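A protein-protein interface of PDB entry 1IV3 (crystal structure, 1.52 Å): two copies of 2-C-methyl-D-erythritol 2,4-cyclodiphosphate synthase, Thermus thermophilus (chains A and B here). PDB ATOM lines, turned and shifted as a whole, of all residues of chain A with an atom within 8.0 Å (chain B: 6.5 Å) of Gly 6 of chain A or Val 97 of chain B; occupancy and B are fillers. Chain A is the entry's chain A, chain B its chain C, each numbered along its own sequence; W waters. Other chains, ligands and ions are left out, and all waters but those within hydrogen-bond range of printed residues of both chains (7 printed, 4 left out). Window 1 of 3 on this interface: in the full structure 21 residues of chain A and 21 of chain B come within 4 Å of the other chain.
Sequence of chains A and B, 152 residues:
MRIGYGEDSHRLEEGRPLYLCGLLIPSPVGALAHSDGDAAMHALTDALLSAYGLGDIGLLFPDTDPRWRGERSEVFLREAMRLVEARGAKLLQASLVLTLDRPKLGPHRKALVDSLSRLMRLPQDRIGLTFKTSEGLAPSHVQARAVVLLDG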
ATOM      1  N   ILE A   3     -34.172  23.855  35.689  1.00  0.00           N
ATOM      2  CA  ILE A   3     -32.972  23.835  34.862  1.00  0.00           C
ATOM      3  C   ILE A   3     -33.026  22.627  33.934  1.00  0.00           C
ATOM      4  O   ILE A   3     -33.652  21.630  34.306  1.00  0.00           O
ATOM      5  CB  ILE A   3     -31.669  23.794  35.678  1.00  0.00           C
ATOM      6  CG1 ILE A   3     -30.428  23.795  34.778  1.00  0.00           C
ATOM      7  CG2 ILE A   3     -31.607  22.606  36.617  1.00  0.00           C
ATOM      8  CD1 ILE A   3     -29.204  24.414  35.386  1.00  0.00           C
ATOM      9  N   GLY A   4     -32.392  22.750  32.773  1.00  0.00           N
ATOM     10  CA  GLY A   4     -32.368  21.575  31.892  1.00  0.00           C
ATOM     11  C   GLY A   4     -31.002  21.499  31.212  1.00  0.00           C
ATOM     12  O   GLY A   4     -30.427  22.544  30.924  1.00  0.00           O
ATOM     13  N   TYR A   5     -30.513  20.276  30.993  1.00  0.00           N
ATOM     14  CA  TYR A   5     -29.207  20.108  30.364  1.00  0.00           C
ATOM     15  C   TYR A   5     -29.351  19.178  29.180  1.00  0.00           C
ATOM     16  O   TYR A   5     -29.989  18.137  29.335  1.00  0.00           O
ATOM     17  CB  TYR A   5     -28.231  19.554  31.410  1.00  0.00           C
ATOM     18  CG  TYR A   5     -26.842  19.360  30.862  1.00  0.00           C
ATOM     19  CD1 TYR A   5     -26.068  20.471  30.533  1.00  0.00           C
ATOM     20  CD2 TYR A   5     -26.344  18.070  30.694  1.00  0.00           C
ATOM     21  CE1 TYR A   5     -24.788  20.274  30.032  1.00  0.00           C
ATOM     22  CE2 TYR A   5     -25.065  17.879  30.188  1.00  0.00           C
ATOM     23  CZ  TYR A   5     -24.313  18.985  29.864  1.00  0.00           C
ATOM     24  OH  TYR A   5     -23.035  18.796  29.362  1.00  0.00           O
ATOM     25  N   GLY A   6     -28.789  19.479  28.018  1.00  0.00           N
ATOM     26  CA  GLY A   6     -28.837  18.534  26.911  1.00  0.00           C
ATOM     27  C   GLY A   6     -27.571  18.636  26.067  1.00  0.00           C
ATOM     28  O   GLY A   6     -26.818  19.607  26.139  1.00  0.00           O
ATOM     29  N   GLU A   7     -27.382  17.582  25.290  1.00  0.00           N
ATOM     30  CA  GLU A   7     -26.218  17.383  24.467  1.00  0.00           C
ATOM     31  C   GLU A   7     -26.634  16.791  23.119  1.00  0.00           C
ATOM     32  O   GLU A   7     -27.652  16.108  23.029  1.00  0.00           O
ATOM     33  CB  GLU A   7     -25.226  16.391  25.075  1.00  0.00           C
ATOM     34  CG  GLU A   7     -24.662  16.713  26.446  1.00  0.00           C
ATOM     35  CD  GLU A   7     -23.587  15.658  26.777  1.00  0.00           C
ATOM     36  OE1 GLU A   7     -22.905  15.222  25.825  1.00  0.00           O
ATOM     37  OE2 GLU A   7     -23.419  15.284  27.936  1.00  0.00           O
ATOM     38  N   ASP A   8     -25.823  17.055  22.117  1.00  0.00           N
ATOM     39  CA  ASP A   8     -25.969  16.400  20.821  1.00  0.00           C
ATOM     40  C   ASP A   8     -24.613  16.370  20.122  1.00  0.00           C
ATOM     41  O   ASP A   8     -23.761  17.245  20.310  1.00  0.00           O
ATOM     42  CB  ASP A   8     -26.962  17.111  19.911  1.00  0.00           C
ATOM     43  CG  ASP A   8     -27.365  16.239  18.724  1.00  0.00           C
ATOM     44  OD1 ASP A   8     -27.228  15.004  18.829  1.00  0.00           O
ATOM     45  OD2 ASP A   8     -27.678  16.849  17.682  1.00  0.00           O
ATOM     46  N   ALA A  39     -26.919  20.302  15.691  1.00  0.00           N
ATOM     47  CA  ALA A  39     -26.606  19.899  17.059  1.00  0.00           C
ATOM     48  C   ALA A  39     -27.047  20.925  18.089  1.00  0.00           C
ATOM     49  O   ALA A  39     -27.431  20.587  19.213  1.00  0.00           O
ATOM     50  CB  ALA A  39     -25.107  19.628  17.100  1.00  0.00           C
ATOM     51  N   ALA A  40     -26.968  22.212  17.749  1.00  0.00           N
ATOM     52  CA  ALA A  40     -27.414  23.300  18.613  1.00  0.00           C
ATOM     53  C   ALA A  40     -28.904  23.147  18.908  1.00  0.00           C
ATOM     54  O   ALA A  40     -29.350  23.102  20.046  1.00  0.00           O
ATOM     55  CB  ALA A  40     -27.195  24.669  17.973  1.00  0.00           C
ATOM     56  N   HIS A  42     -30.718  20.506  18.519  1.00  0.00           N
ATOM     57  CA  HIS A  42     -31.056  19.272  19.235  1.00  0.00           C
ATOM     58  C   HIS A  42     -30.733  19.350  20.724  1.00  0.00           C
ATOM     59  O   HIS A  42     -31.548  18.934  21.549  1.00  0.00           O
ATOM     60  CB  HIS A  42     -30.313  18.079  18.637  1.00  0.00           C
ATOM     61  CG  HIS A  42     -30.845  17.739  17.286  1.00  0.00           C
ATOM     62  ND1 HIS A  42     -30.345  16.740  16.497  1.00  0.00           N
ATOM     63  CD2 HIS A  42     -31.875  18.302  16.595  1.00  0.00           C
ATOM     64  CE1 HIS A  42     -31.029  16.682  15.363  1.00  0.00           C
ATOM     65  NE2 HIS A  42     -31.962  17.623  15.398  1.00  0.00           N
ATOM     66  N   ALA A  43     -29.568  19.918  21.016  1.00  0.00           N
ATOM     67  CA  ALA A  43     -29.193  20.004  22.440  1.00  0.00           C
ATOM     68  C   ALA A  43     -30.104  20.952  23.208  1.00  0.00           C
ATOM     69  O   ALA A  43     -30.447  20.690  24.362  1.00  0.00           O
ATOM     70  CB  ALA A  43     -27.737  20.442  22.563  1.00  0.00           C
ATOM     71  N   LEU A  44     -30.511  22.072  22.593  1.00  0.00           N
ATOM     72  CA  LEU A  44     -31.443  22.997  23.242  1.00  0.00           C
ATOM     73  C   LEU A  44     -32.789  22.326  23.453  1.00  0.00           C
ATOM     74  O   LEU A  44     -33.441  22.495  24.483  1.00  0.00           O
ATOM     75  CB  LEU A  44     -31.631  24.273  22.392  1.00  0.00           C
ATOM     76  CG  LEU A  44     -30.413  25.201  22.393  1.00  0.00           C
ATOM     77  CD1 LEU A  44     -30.479  26.252  21.292  1.00  0.00           C
ATOM     78  CD2 LEU A  44     -30.278  25.847  23.771  1.00  0.00           C
ATOM     79  N   THR A  45     -33.220  21.547  22.456  1.00  0.00           N
ATOM     80  CA  THR A  45     -34.543  20.906  22.558  1.00  0.00           C
ATOM     81  C   THR A  45     -34.545  19.869  23.687  1.00  0.00           C
ATOM     82  O   THR A  45     -35.456  19.808  24.531  1.00  0.00           O
ATOM     83  CB  THR A  45     -34.928  20.243  21.228  1.00  0.00           C
ATOM     84  OG1 THR A  45     -34.959  21.196  20.153  1.00  0.00           O
ATOM     85  CG2 THR A  45     -36.346  19.673  21.299  1.00  0.00           C
ATOM     86  N   ASP A  46     -33.502  19.035  23.707  1.00  0.00           N
ATOM     87  CA  ASP A  46     -33.376  18.074  24.806  1.00  0.00           C
ATOM     88  C   ASP A  46     -33.309  18.792  26.159  1.00  0.00           C
ATOM     89  O   ASP A  46     -33.903  18.331  27.134  1.00  0.00           O
ATOM     90  CB  ASP A  46     -32.157  17.173  24.641  1.00  0.00           C
ATOM     91  CG  ASP A  46     -32.405  15.918  23.821  1.00  0.00           C
ATOM     92  OD1 ASP A  46     -33.585  15.629  23.520  1.00  0.00           O
ATOM     93  OD2 ASP A  46     -31.437  15.193  23.492  1.00  0.00           O
ATOM     94  N   ALA A  47     -32.584  19.905  26.263  1.00  0.00           N
ATOM     95  CA  ALA A  47     -32.477  20.613  27.537  1.00  0.00           C
ATOM     96  C   ALA A  47     -33.840  21.109  28.004  1.00  0.00           C
ATOM     97  O   ALA A  47     -34.178  21.004  29.187  1.00  0.00           O
ATOM     98  CB  ALA A  47     -31.503  21.781  27.417  1.00  0.00           C
ATOM     99  N   LEU A  48     -34.640  21.675  27.073  1.00  0.00           N
ATOM    100  CA  LEU A  48     -35.998  22.113  27.399  1.00  0.00           C
ATOM    101  C   LEU A  48     -36.866  20.966  27.867  1.00  0.00           C
ATOM    102  O   LEU A  48     -37.552  21.060  28.892  1.00  0.00           O
ATOM    103  CB  LEU A  48     -36.629  22.764  26.159  1.00  0.00           C
ATOM    104  CG  LEU A  48     -36.043  24.117  25.738  1.00  0.00           C
ATOM    105  CD1 LEU A  48     -36.612  24.552  24.378  1.00  0.00           C
ATOM    106  CD2 LEU A  48     -36.325  25.215  26.765  1.00  0.00           C
ATOM    107  N   SER A  50     -35.929  18.130  29.023  1.00  0.00           N
ATOM    108  CA  SER A  50     -35.330  17.664  30.270  1.00  0.00           C
ATOM    109  C   SER A  50     -35.794  18.481  31.476  1.00  0.00           C
ATOM    110  O   SER A  50     -36.005  17.925  32.560  1.00  0.00           O
ATOM    111  CB  SER A  50     -33.797  17.718  30.136  1.00  0.00           C
ATOM    112  OG  SER A  50     -33.229  16.879  31.142  1.00  0.00           O
ATOM    113  N   ALA A  51     -35.939  19.791  31.293  1.00  0.00           N
ATOM    114  CA  ALA A  51     -36.337  20.662  32.392  1.00  0.00           C
ATOM    115  C   ALA A  51     -37.703  20.280  32.965  1.00  0.00           C
ATOM    116  O   ALA A  51     -38.004  20.692  34.086  1.00  0.00           O
ATOM    117  CB  ALA A  51     -36.362  22.123  31.972  1.00  0.00           C
ATOM    118  N   ASP A  56     -36.912  12.997  25.564  1.00  0.00           N
ATOM    119  CA  ASP A  56     -35.847  13.572  24.739  1.00  0.00           C
ATOM    120  C   ASP A  56     -36.310  13.517  23.286  1.00  0.00           C
ATOM    121  O   ASP A  56     -37.428  13.060  22.983  1.00  0.00           O
ATOM    122  CB  ASP A  56     -34.507  12.885  24.970  1.00  0.00           C
ATOM    123  CG  ASP A  56     -34.503  11.407  24.693  1.00  0.00           C
ATOM    124  OD1 ASP A  56     -35.097  10.998  23.678  1.00  0.00           O
ATOM    125  OD2 ASP A  56     -33.903  10.586  25.417  1.00  0.00           O
ATOM    126  N   SER A  95     -27.701  28.804  27.510  1.00  0.00           N
ATOM    127  CA  SER A  95     -26.258  28.962  27.426  1.00  0.00           C
ATOM    128  C   SER A  95     -25.705  27.694  26.808  1.00  0.00           C
ATOM    129  O   SER A  95     -25.961  26.625  27.368  1.00  0.00           O
ATOM    130  CB  SER A  95     -25.655  29.185  28.818  1.00  0.00           C
ATOM    131  OG  SER A  95     -24.247  29.375  28.690  1.00  0.00           O
ATOM    132  N   LEU A  96     -25.007  27.807  25.676  1.00  0.00           N
ATOM    133  CA  LEU A  96     -24.540  26.556  25.074  1.00  0.00           C
ATOM    134  C   LEU A  96     -23.189  26.721  24.397  1.00  0.00           C
ATOM    135  O   LEU A  96     -22.814  27.834  24.044  1.00  0.00           O
ATOM    136  CB  LEU A  96     -25.539  26.046  24.041  1.00  0.00           C
ATOM    137  CG  LEU A  96     -25.671  26.897  22.778  1.00  0.00           C
ATOM    138  CD1 LEU A  96     -26.335  26.111  21.653  1.00  0.00           C
ATOM    139  CD2 LEU A  96     -26.498  28.146  23.064  1.00  0.00           C
ATOM    140  N   VAL A  97     -22.537  25.567  24.244  1.00  0.00           N
ATOM    141  CA  VAL A  97     -21.239  25.528  23.589  1.00  0.00           C
ATOM    142  C   VAL A  97     -21.330  24.635  22.355  1.00  0.00           C
ATOM    143  O   VAL A  97     -21.823  23.511  22.435  1.00  0.00           O
ATOM    144  CB  VAL A  97     -20.155  24.933  24.499  1.00  0.00           C
ATOM    145  CG1 VAL A  97     -18.784  24.967  23.860  1.00  0.00           C
ATOM    146  CG2 VAL A  97     -20.130  25.694  25.832  1.00  0.00           C
ATOM    147  N   ALA A 144     -22.626  19.758  20.629  1.00  0.00           N
ATOM    148  CA  ALA A 144     -23.263  20.874  21.315  1.00  0.00           C
ATOM    149  C   ALA A 144     -23.614  20.422  22.724  1.00  0.00           C
ATOM    150  O   ALA A 144     -24.040  19.276  22.873  1.00  0.00           O
ATOM    151  CB  ALA A 144     -24.534  21.348  20.617  1.00  0.00           C
ATOM    152  N   ARG A 145     -23.456  21.310  23.699  1.00  0.00           N
ATOM    153  CA  ARG A 145     -23.988  21.058  25.041  1.00  0.00           C
ATOM    154  C   ARG A 145     -24.656  22.334  25.513  1.00  0.00           C
ATOM    155  O   ARG A 145     -24.110  23.423  25.278  1.00  0.00           O
ATOM    156  CB  ARG A 145     -22.888  20.600  26.003  1.00  0.00           C
ATOM    157  CG  ARG A 145     -22.123  19.385  25.475  1.00  0.00           C
ATOM    158  CD  ARG A 145     -21.148  18.846  26.525  1.00  0.00           C
ATOM    159  NE  ARG A 145     -20.650  17.537  26.071  1.00  0.00           N
ATOM    160  CZ  ARG A 145     -19.598  17.484  25.260  1.00  0.00           C
ATOM    161  NH1 ARG A 145     -19.010  18.614  24.893  1.00  0.00           N
ATOM    162  NH2 ARG A 145     -19.153  16.308  24.848  1.00  0.00           N
ATOM    163  N   ALA A 146     -25.835  22.182  26.119  1.00  0.00           N
ATOM    164  CA  ALA A 146     -26.667  23.327  26.436  1.00  0.00           C
ATOM    165  C   ALA A 146     -27.275  23.233  27.837  1.00  0.00           C
ATOM    166  O   ALA A 146     -27.671  22.128  28.207  1.00  0.00           O
ATOM    167  CB  ALA A 146     -27.829  23.487  25.449  1.00  0.00           C
ATOM    168  N   VAL A 147     -27.357  24.379  28.516  1.00  0.00           N
ATOM    169  CA  VAL A 147     -28.136  24.471  29.765  1.00  0.00           C
ATOM    170  C   VAL A 147     -29.232  25.505  29.549  1.00  0.00           C
ATOM    171  O   VAL A 147     -28.977  26.579  28.970  1.00  0.00           O
ATOM    172  CB  VAL A 147     -27.271  24.867  30.974  1.00  0.00           C
ATOM    173  CG1 VAL A 147     -28.009  24.792  32.288  1.00  0.00           C
ATOM    174  CG2 VAL A 147     -26.049  23.950  31.070  1.00  0.00           C
ATOM    175  N   VAL A 148     -30.438  25.205  29.987  1.00  0.00           N
ATOM    176  CA  VAL A 148     -31.480  26.241  29.916  1.00  0.00           C
ATOM    177  C   VAL A 148     -31.978  26.511  31.332  1.00  0.00           C
ATOM    178  O   VAL A 148     -31.930  25.657  32.240  1.00  0.00           O
ATOM    179  CB  VAL A 148     -32.667  25.853  29.015  1.00  0.00           C
ATOM    180  CG1 VAL A 148     -32.245  25.718  27.561  1.00  0.00           C
ATOM    181  CG2 VAL A 148     -33.286  24.559  29.521  1.00  0.00           C
ATOM    182  N   SER B  95     -30.784  16.986  36.160  1.00  0.00           N
ATOM    183  CA  SER B  95     -30.943  16.888  34.704  1.00  0.00           C
ATOM    184  C   SER B  95     -29.660  16.283  34.173  1.00  0.00           C
ATOM    185  O   SER B  95     -28.608  16.889  34.447  1.00  0.00           O
ATOM    186  CB  SER B  95     -31.201  18.251  34.063  1.00  0.00           C
ATOM    187  OG  SER B  95     -31.340  18.136  32.640  1.00  0.00           O
ATOM    188  N   LEU B  96     -29.753  15.160  33.477  1.00  0.00           N
ATOM    189  CA  LEU B  96     -28.495  14.531  33.043  1.00  0.00           C
ATOM    190  C   LEU B  96     -28.638  13.844  31.688  1.00  0.00           C
ATOM    191  O   LEU B  96     -29.742  13.490  31.295  1.00  0.00           O
ATOM    192  CB  LEU B  96     -27.992  13.516  34.087  1.00  0.00           C
ATOM    193  CG  LEU B  96     -28.766  12.199  34.136  1.00  0.00           C
ATOM    194  CD1 LEU B  96     -27.975  11.179  34.961  1.00  0.00           C
ATOM    195  CD2 LEU B  96     -30.140  12.408  34.738  1.00  0.00           C
ATOM    196  N   VAL B  97     -27.500  13.684  31.017  1.00  0.00           N
ATOM    197  CA  VAL B  97     -27.464  13.060  29.696  1.00  0.00           C
ATOM    198  C   VAL B  97     -26.602  11.809  29.763  1.00  0.00           C
ATOM    199  O   VAL B  97     -25.465  11.918  30.227  1.00  0.00           O
ATOM    200  CB  VAL B  97     -26.876  14.012  28.634  1.00  0.00           C
ATOM    201  CG1 VAL B  97     -26.930  13.414  27.232  1.00  0.00           C
ATOM    202  CG2 VAL B  97     -27.617  15.348  28.675  1.00  0.00           C
ATOM    203  N   LEU B  98     -27.133  10.678  29.311  1.00  0.00           N
ATOM    204  CA  LEU B  98     -26.292   9.494  29.219  1.00  0.00           C
ATOM    205  C   LEU B  98     -25.923   9.269  27.754  1.00  0.00           C
ATOM    206  O   LEU B  98     -26.852   9.336  26.930  1.00  0.00           O
ATOM    207  CB  LEU B  98     -26.982   8.251  29.780  1.00  0.00           C
ATOM    208  CG  LEU B  98     -27.651   8.436  31.133  1.00  0.00           C
ATOM    209  CD1 LEU B  98     -28.287   7.130  31.595  1.00  0.00           C
ATOM    210  CD2 LEU B  98     -26.629   8.946  32.140  1.00  0.00           C
ATOM    211  N   THR B  99     -24.659   9.007  27.483  1.00  0.00           N
ATOM    212  CA  THR B  99     -24.203   8.709  26.132  1.00  0.00           C
ATOM    213  C   THR B  99     -23.550   7.335  26.046  1.00  0.00           C
ATOM    214  O   THR B  99     -22.632   7.032  26.798  1.00  0.00           O
ATOM    215  CB  THR B  99     -23.193   9.761  25.648  1.00  0.00           C
ATOM    216  OG1 THR B  99     -23.823  11.027  25.839  1.00  0.00           O
ATOM    217  CG2 THR B  99     -22.916   9.666  24.159  1.00  0.00           C
ATOM    218  N   GLY B 128     -34.698  14.988  34.908  1.00  0.00           N
ATOM    219  CA  GLY B 128     -34.588  15.218  33.460  1.00  0.00           C
ATOM    220  C   GLY B 128     -33.529  14.303  32.875  1.00  0.00           C
ATOM    221  O   GLY B 128     -32.335  14.630  32.931  1.00  0.00           O
ATOM    222  N   LEU B 129     -33.933  13.155  32.343  1.00  0.00           N
ATOM    223  CA  LEU B 129     -32.978  12.182  31.825  1.00  0.00           C
ATOM    224  C   LEU B 129     -33.097  12.123  30.312  1.00  0.00           C
ATOM    225  O   LEU B 129     -34.209  11.943  29.824  1.00  0.00           O
ATOM    226  CB  LEU B 129     -33.225  10.819  32.463  1.00  0.00           C
ATOM    227  CG  LEU B 129     -32.405   9.613  32.029  1.00  0.00           C
ATOM    228  CD1 LEU B 129     -30.909   9.712  32.336  1.00  0.00           C
ATOM    229  CD2 LEU B 129     -32.960   8.348  32.701  1.00  0.00           C
ATOM    230  N   THR B 130     -31.995  12.278  29.590  1.00  0.00           N
ATOM    231  CA  THR B 130     -32.037  12.139  28.134  1.00  0.00           C
ATOM    232  C   THR B 130     -30.945  11.180  27.685  1.00  0.00           C
ATOM    233  O   THR B 130     -29.876  11.020  28.300  1.00  0.00           O
ATOM    234  CB  THR B 130     -31.924  13.511  27.427  1.00  0.00           C
ATOM    235  OG1 THR B 130     -30.684  14.122  27.792  1.00  0.00           O
ATOM    236  CG2 THR B 130     -33.013  14.479  27.882  1.00  0.00           C
ATOM    237  N   PHE B 131     -31.184  10.479  26.574  1.00  0.00           N
ATOM    238  CA  PHE B 131     -30.238   9.477  26.099  1.00  0.00           C
ATOM    239  C   PHE B 131     -29.641   9.854  24.745  1.00  0.00           C
ATOM    240  O   PHE B 131     -30.403  10.317  23.888  1.00  0.00           O
ATOM    241  CB  PHE B 131     -30.954   8.140  25.886  1.00  0.00           C
ATOM    242  CG  PHE B 131     -31.742   7.660  27.085  1.00  0.00           C
ATOM    243  CD1 PHE B 131     -31.189   7.769  28.347  1.00  0.00           C
ATOM    244  CD2 PHE B 131     -33.002   7.113  26.912  1.00  0.00           C
ATOM    245  CE1 PHE B 131     -31.881   7.321  29.456  1.00  0.00           C
ATOM    246  CE2 PHE B 131     -33.682   6.659  28.024  1.00  0.00           C
ATOM    247  CZ  PHE B 131     -33.125   6.749  29.292  1.00  0.00           C
ATOM    248  N   LYS B 132     -28.357   9.644  24.544  1.00  0.00           N
ATOM    249  CA  LYS B 132     -27.713   9.888  23.259  1.00  0.00           C
ATOM    250  C   LYS B 132     -26.810   8.712  22.892  1.00  0.00           C
ATOM    251  O   LYS B 132     -26.402   7.985  23.808  1.00  0.00           O
ATOM    252  CB  LYS B 132     -26.890  11.181  23.326  1.00  0.00           C
ATOM    253  CG  LYS B 132     -27.647  12.402  23.852  1.00  0.00           C
ATOM    254  CD  LYS B 132     -28.653  12.863  22.782  1.00  0.00           C
ATOM    255  CE  LYS B 132     -27.919  12.982  21.447  1.00  0.00           C
ATOM    256  NZ  LYS B 132     -28.854  13.345  20.336  1.00  0.00           N
ATOM    257  N   GLN B 143     -20.925   7.406  29.028  1.00  0.00           N
ATOM    258  CA  GLN B 143     -20.631   8.731  29.556  1.00  0.00           C
ATOM    259  C   GLN B 143     -21.876   9.342  30.181  1.00  0.00           C
ATOM    260  O   GLN B 143     -22.983   9.089  29.693  1.00  0.00           O
ATOM    261  CB  GLN B 143     -20.151   9.706  28.482  1.00  0.00           C
ATOM    262  CG  GLN B 143     -18.970   9.200  27.670  1.00  0.00           C
ATOM    263  CD  GLN B 143     -18.751  10.080  26.450  1.00  0.00           C
ATOM    264  OE1 GLN B 143     -19.122   9.719  25.329  1.00  0.00           O
ATOM    265  NE2 GLN B 143     -18.156  11.242  26.689  1.00  0.00           N
ATOM    266  N   ALA B 144     -21.641  10.129  31.228  1.00  0.00           N
ATOM    267  CA  ALA B 144     -22.759  10.807  31.874  1.00  0.00           C
ATOM    268  C   ALA B 144     -22.332  12.203  32.324  1.00  0.00           C
ATOM    269  O   ALA B 144     -21.218  12.379  32.810  1.00  0.00           O
ATOM    270  CB  ALA B 144     -23.302  10.067  33.089  1.00  0.00           C
ATOM    271  N   ARG B 145     -23.252  13.143  32.142  1.00  0.00           N
ATOM    272  CA  ARG B 145     -22.996  14.527  32.573  1.00  0.00           C
ATOM    273  C   ARG B 145     -24.272  15.044  33.233  1.00  0.00           C
ATOM    274  O   ARG B 145     -25.352  14.887  32.672  1.00  0.00           O
ATOM    275  CB  ARG B 145     -22.536  15.432  31.427  1.00  0.00           C
ATOM    276  CG  ARG B 145     -21.184  14.976  30.872  1.00  0.00           C
ATOM    277  CD  ARG B 145     -20.548  15.954  29.886  1.00  0.00           C
ATOM    278  NE  ARG B 145     -19.413  15.253  29.275  1.00  0.00           N
ATOM    279  CZ  ARG B 145     -19.477  14.506  28.184  1.00  0.00           C
ATOM    280  NH1 ARG B 145     -20.581  14.300  27.479  1.00  0.00           N
ATOM    281  NH2 ARG B 145     -18.339  13.943  27.784  1.00  0.00           N
ATOM    282  N   ALA B 146     -24.099  15.616  34.428  1.00  0.00           N
ATOM    283  CA  ALA B 146     -25.324  15.934  35.184  1.00  0.00           C
ATOM    284  C   ALA B 146     -25.274  17.320  35.794  1.00  0.00           C
ATOM    285  O   ALA B 146     -24.199  17.774  36.238  1.00  0.00           O
ATOM    286  CB  ALA B 146     -25.523  14.900  36.290  1.00  0.00           C
HETATM  287  O   HOH W   1     -33.026   9.053  22.936  1.00  0.00           O
HETATM  288  O   HOH W   2     -29.515  15.420  25.472  1.00  0.00           O
HETATM  289  O   HOH W   3     -36.668  17.515  35.237  1.00  0.00           O
HETATM  290  O   HOH W   4     -20.719  13.024  24.854  1.00  0.00           O
HETATM  291  O   HOH W   5     -26.829  12.214  18.454  1.00  0.00           O
HETATM  292  O   HOH W   6     -23.393  12.286  28.206  1.00  0.00           O
HETATM  293  O   HOH W   7     -23.427  13.249  24.343  1.00  0.00           O
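The side-chain hydroxyl (OG) of Ser 95 of chain B is in hydrogen-bond range of the side-chain hydroxyl (OG) of Ser 50 of chain A (2.7 Å).
The backbone carbonyl oxygen (O) of Gly 128 of chain B is in hydrogen-bond range of the side-chain hydroxyl (OG) of Ser 50 of chain A.
The backbone NH (N) of Tyr 5 of chain A sits at hydrogen-bond distance from the side-chain hydroxyl (OG) of Ser 95 of chain B (2.8 Å).
The guanidinium group (NH1) of Arg 145 of chain B is in salt-bridge range of the side-chain carboxylate (OE1) of Glu 7 of chain A.
The side-chain amino group (NZ) of Lys 132 of chain B is in salt-bridge range of the side-chain carboxylate (OD1) of Asp 8 of chain A (2.8 Å).
N of Phe 131 of chain B sits at hydrogen-bond distance from OD2 of Asp 56 of chain A (3.0 Å).
N of Val 97 of chain B lies within hydrogen-bond range of O of Arg 145 of chain B (3.0 Å).
The backbone NH (N) of Thr 130 of chain B is in hydrogen-bond range of the backbone carbonyl oxygen (O) of Leu 96 of chain B, at 3.1 Å.
N of Ala 146 of chain A sits at hydrogen-bond distance from O of Gly 6 of chain A, at 2.8 Å.
N of Lys 132 of chain B sits at hydrogen-bond distance from O of Leu 98 of chain B (2.8 Å).
The backbone carbonyl oxygen (O) of Gly 4 of chain A sits at hydrogen-bond distance from the backbone NH (N) of Val 148 of chain A (2.8 Å).
The backbone NH (N) of Ala 144 of chain A sits at hydrogen-bond distance from the backbone carbonyl oxygen (O) of Asp 8 of chain A (2.8 Å).
Gly 4 of chain A touches Ser 95 of chain B (CA to OG, 3.7 Å).
Tyr 5 of chain A touches Val 97 of chain B (CD2 to CG2, 3.6 Å).
Tyr 5 of chain A touches Arg 145 of chain B.
CA of Gly 6 of chain A touches CG2 of Val 97 of chain B, at 3.8 Å.
OE2 of Glu 7 of chain A touches CB of Val 97 of chain B, 3.7 Å away.
O of Glu 7 of chain A touches CD of Lys 132 of chain B, at 3.4 Å.
Lys 132 of chain B touches Asp 46 of chain A (CD to OD2, 3.7 Å).
Ser 50 of chain A touches Leu 129 of chain B (OG to N, 3.98 Å).
CB of Asp 56 of chain A touches CB of Thr 130 of chain B, 3.6 Å away.
Arg 145 of chain B touches Arg 145 of chain A.
Of the printed residues of chain B, Gly 4 of chain A touches Ser 95.
Of chain B, only Val 97 comes within 4 Å of Gly 6 of chain A.
Printed residues of chain B within 4 Å of Arg 145 of chain A: Arg 145 (3.5 Å).
Of chain A, only Tyr 5, Gly 6 and Glu 7 come within 4 Å of Val 97 of chain B.
Of the printed residues of chain A, Gly 128 of chain B touches Ser 50 (3.0 Å).
Gln 143 of chain B touches none of the printed residues of chain A.
Hydrophobic or aromatic side chains of chain B that line the printed part of chain A: Val 97 and Phe 131.
Among the printed residues, 16 pairs touch across the chains.
Arg 145 of chain B touches its own counterpart, Arg 145 of chain A.
Water W7 lies within hydrogen-bond range of OE1 of Glu 7 of chain A (2.5 Å) and OG1 of Thr 99 of chain B (2.7 Å).
Water W6 lies within hydrogen-bond range of the side-chain hydroxyl (OG1) of Thr 99 of chain B, the backbone carbonyl oxygen (O) of Val 97 of chain B and the side-chain carboxylate (OE2) of Glu 7 of chain A.
Water W2 lies within hydrogen-bond range of OD2 of Asp 46 of chain A (2.8 Å), OG1 of Thr 130 of chain B (2.9 Å) and N of Glu 7 of chain A (3.0 Å).
Water W3 lies within hydrogen-bond range of O of Ser 50 of chain A and N of Gly 128 of chain B.
Water W4 bridges the guanidinium group of Arg 145 of chain B and the side-chain carboxylate of Glu 7 of chain A.
Water W1 lies within hydrogen-bond range of OD1 of Asp 56 of chain A (2.9 Å) and O of Phe 131 of chain B (3.1 Å).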
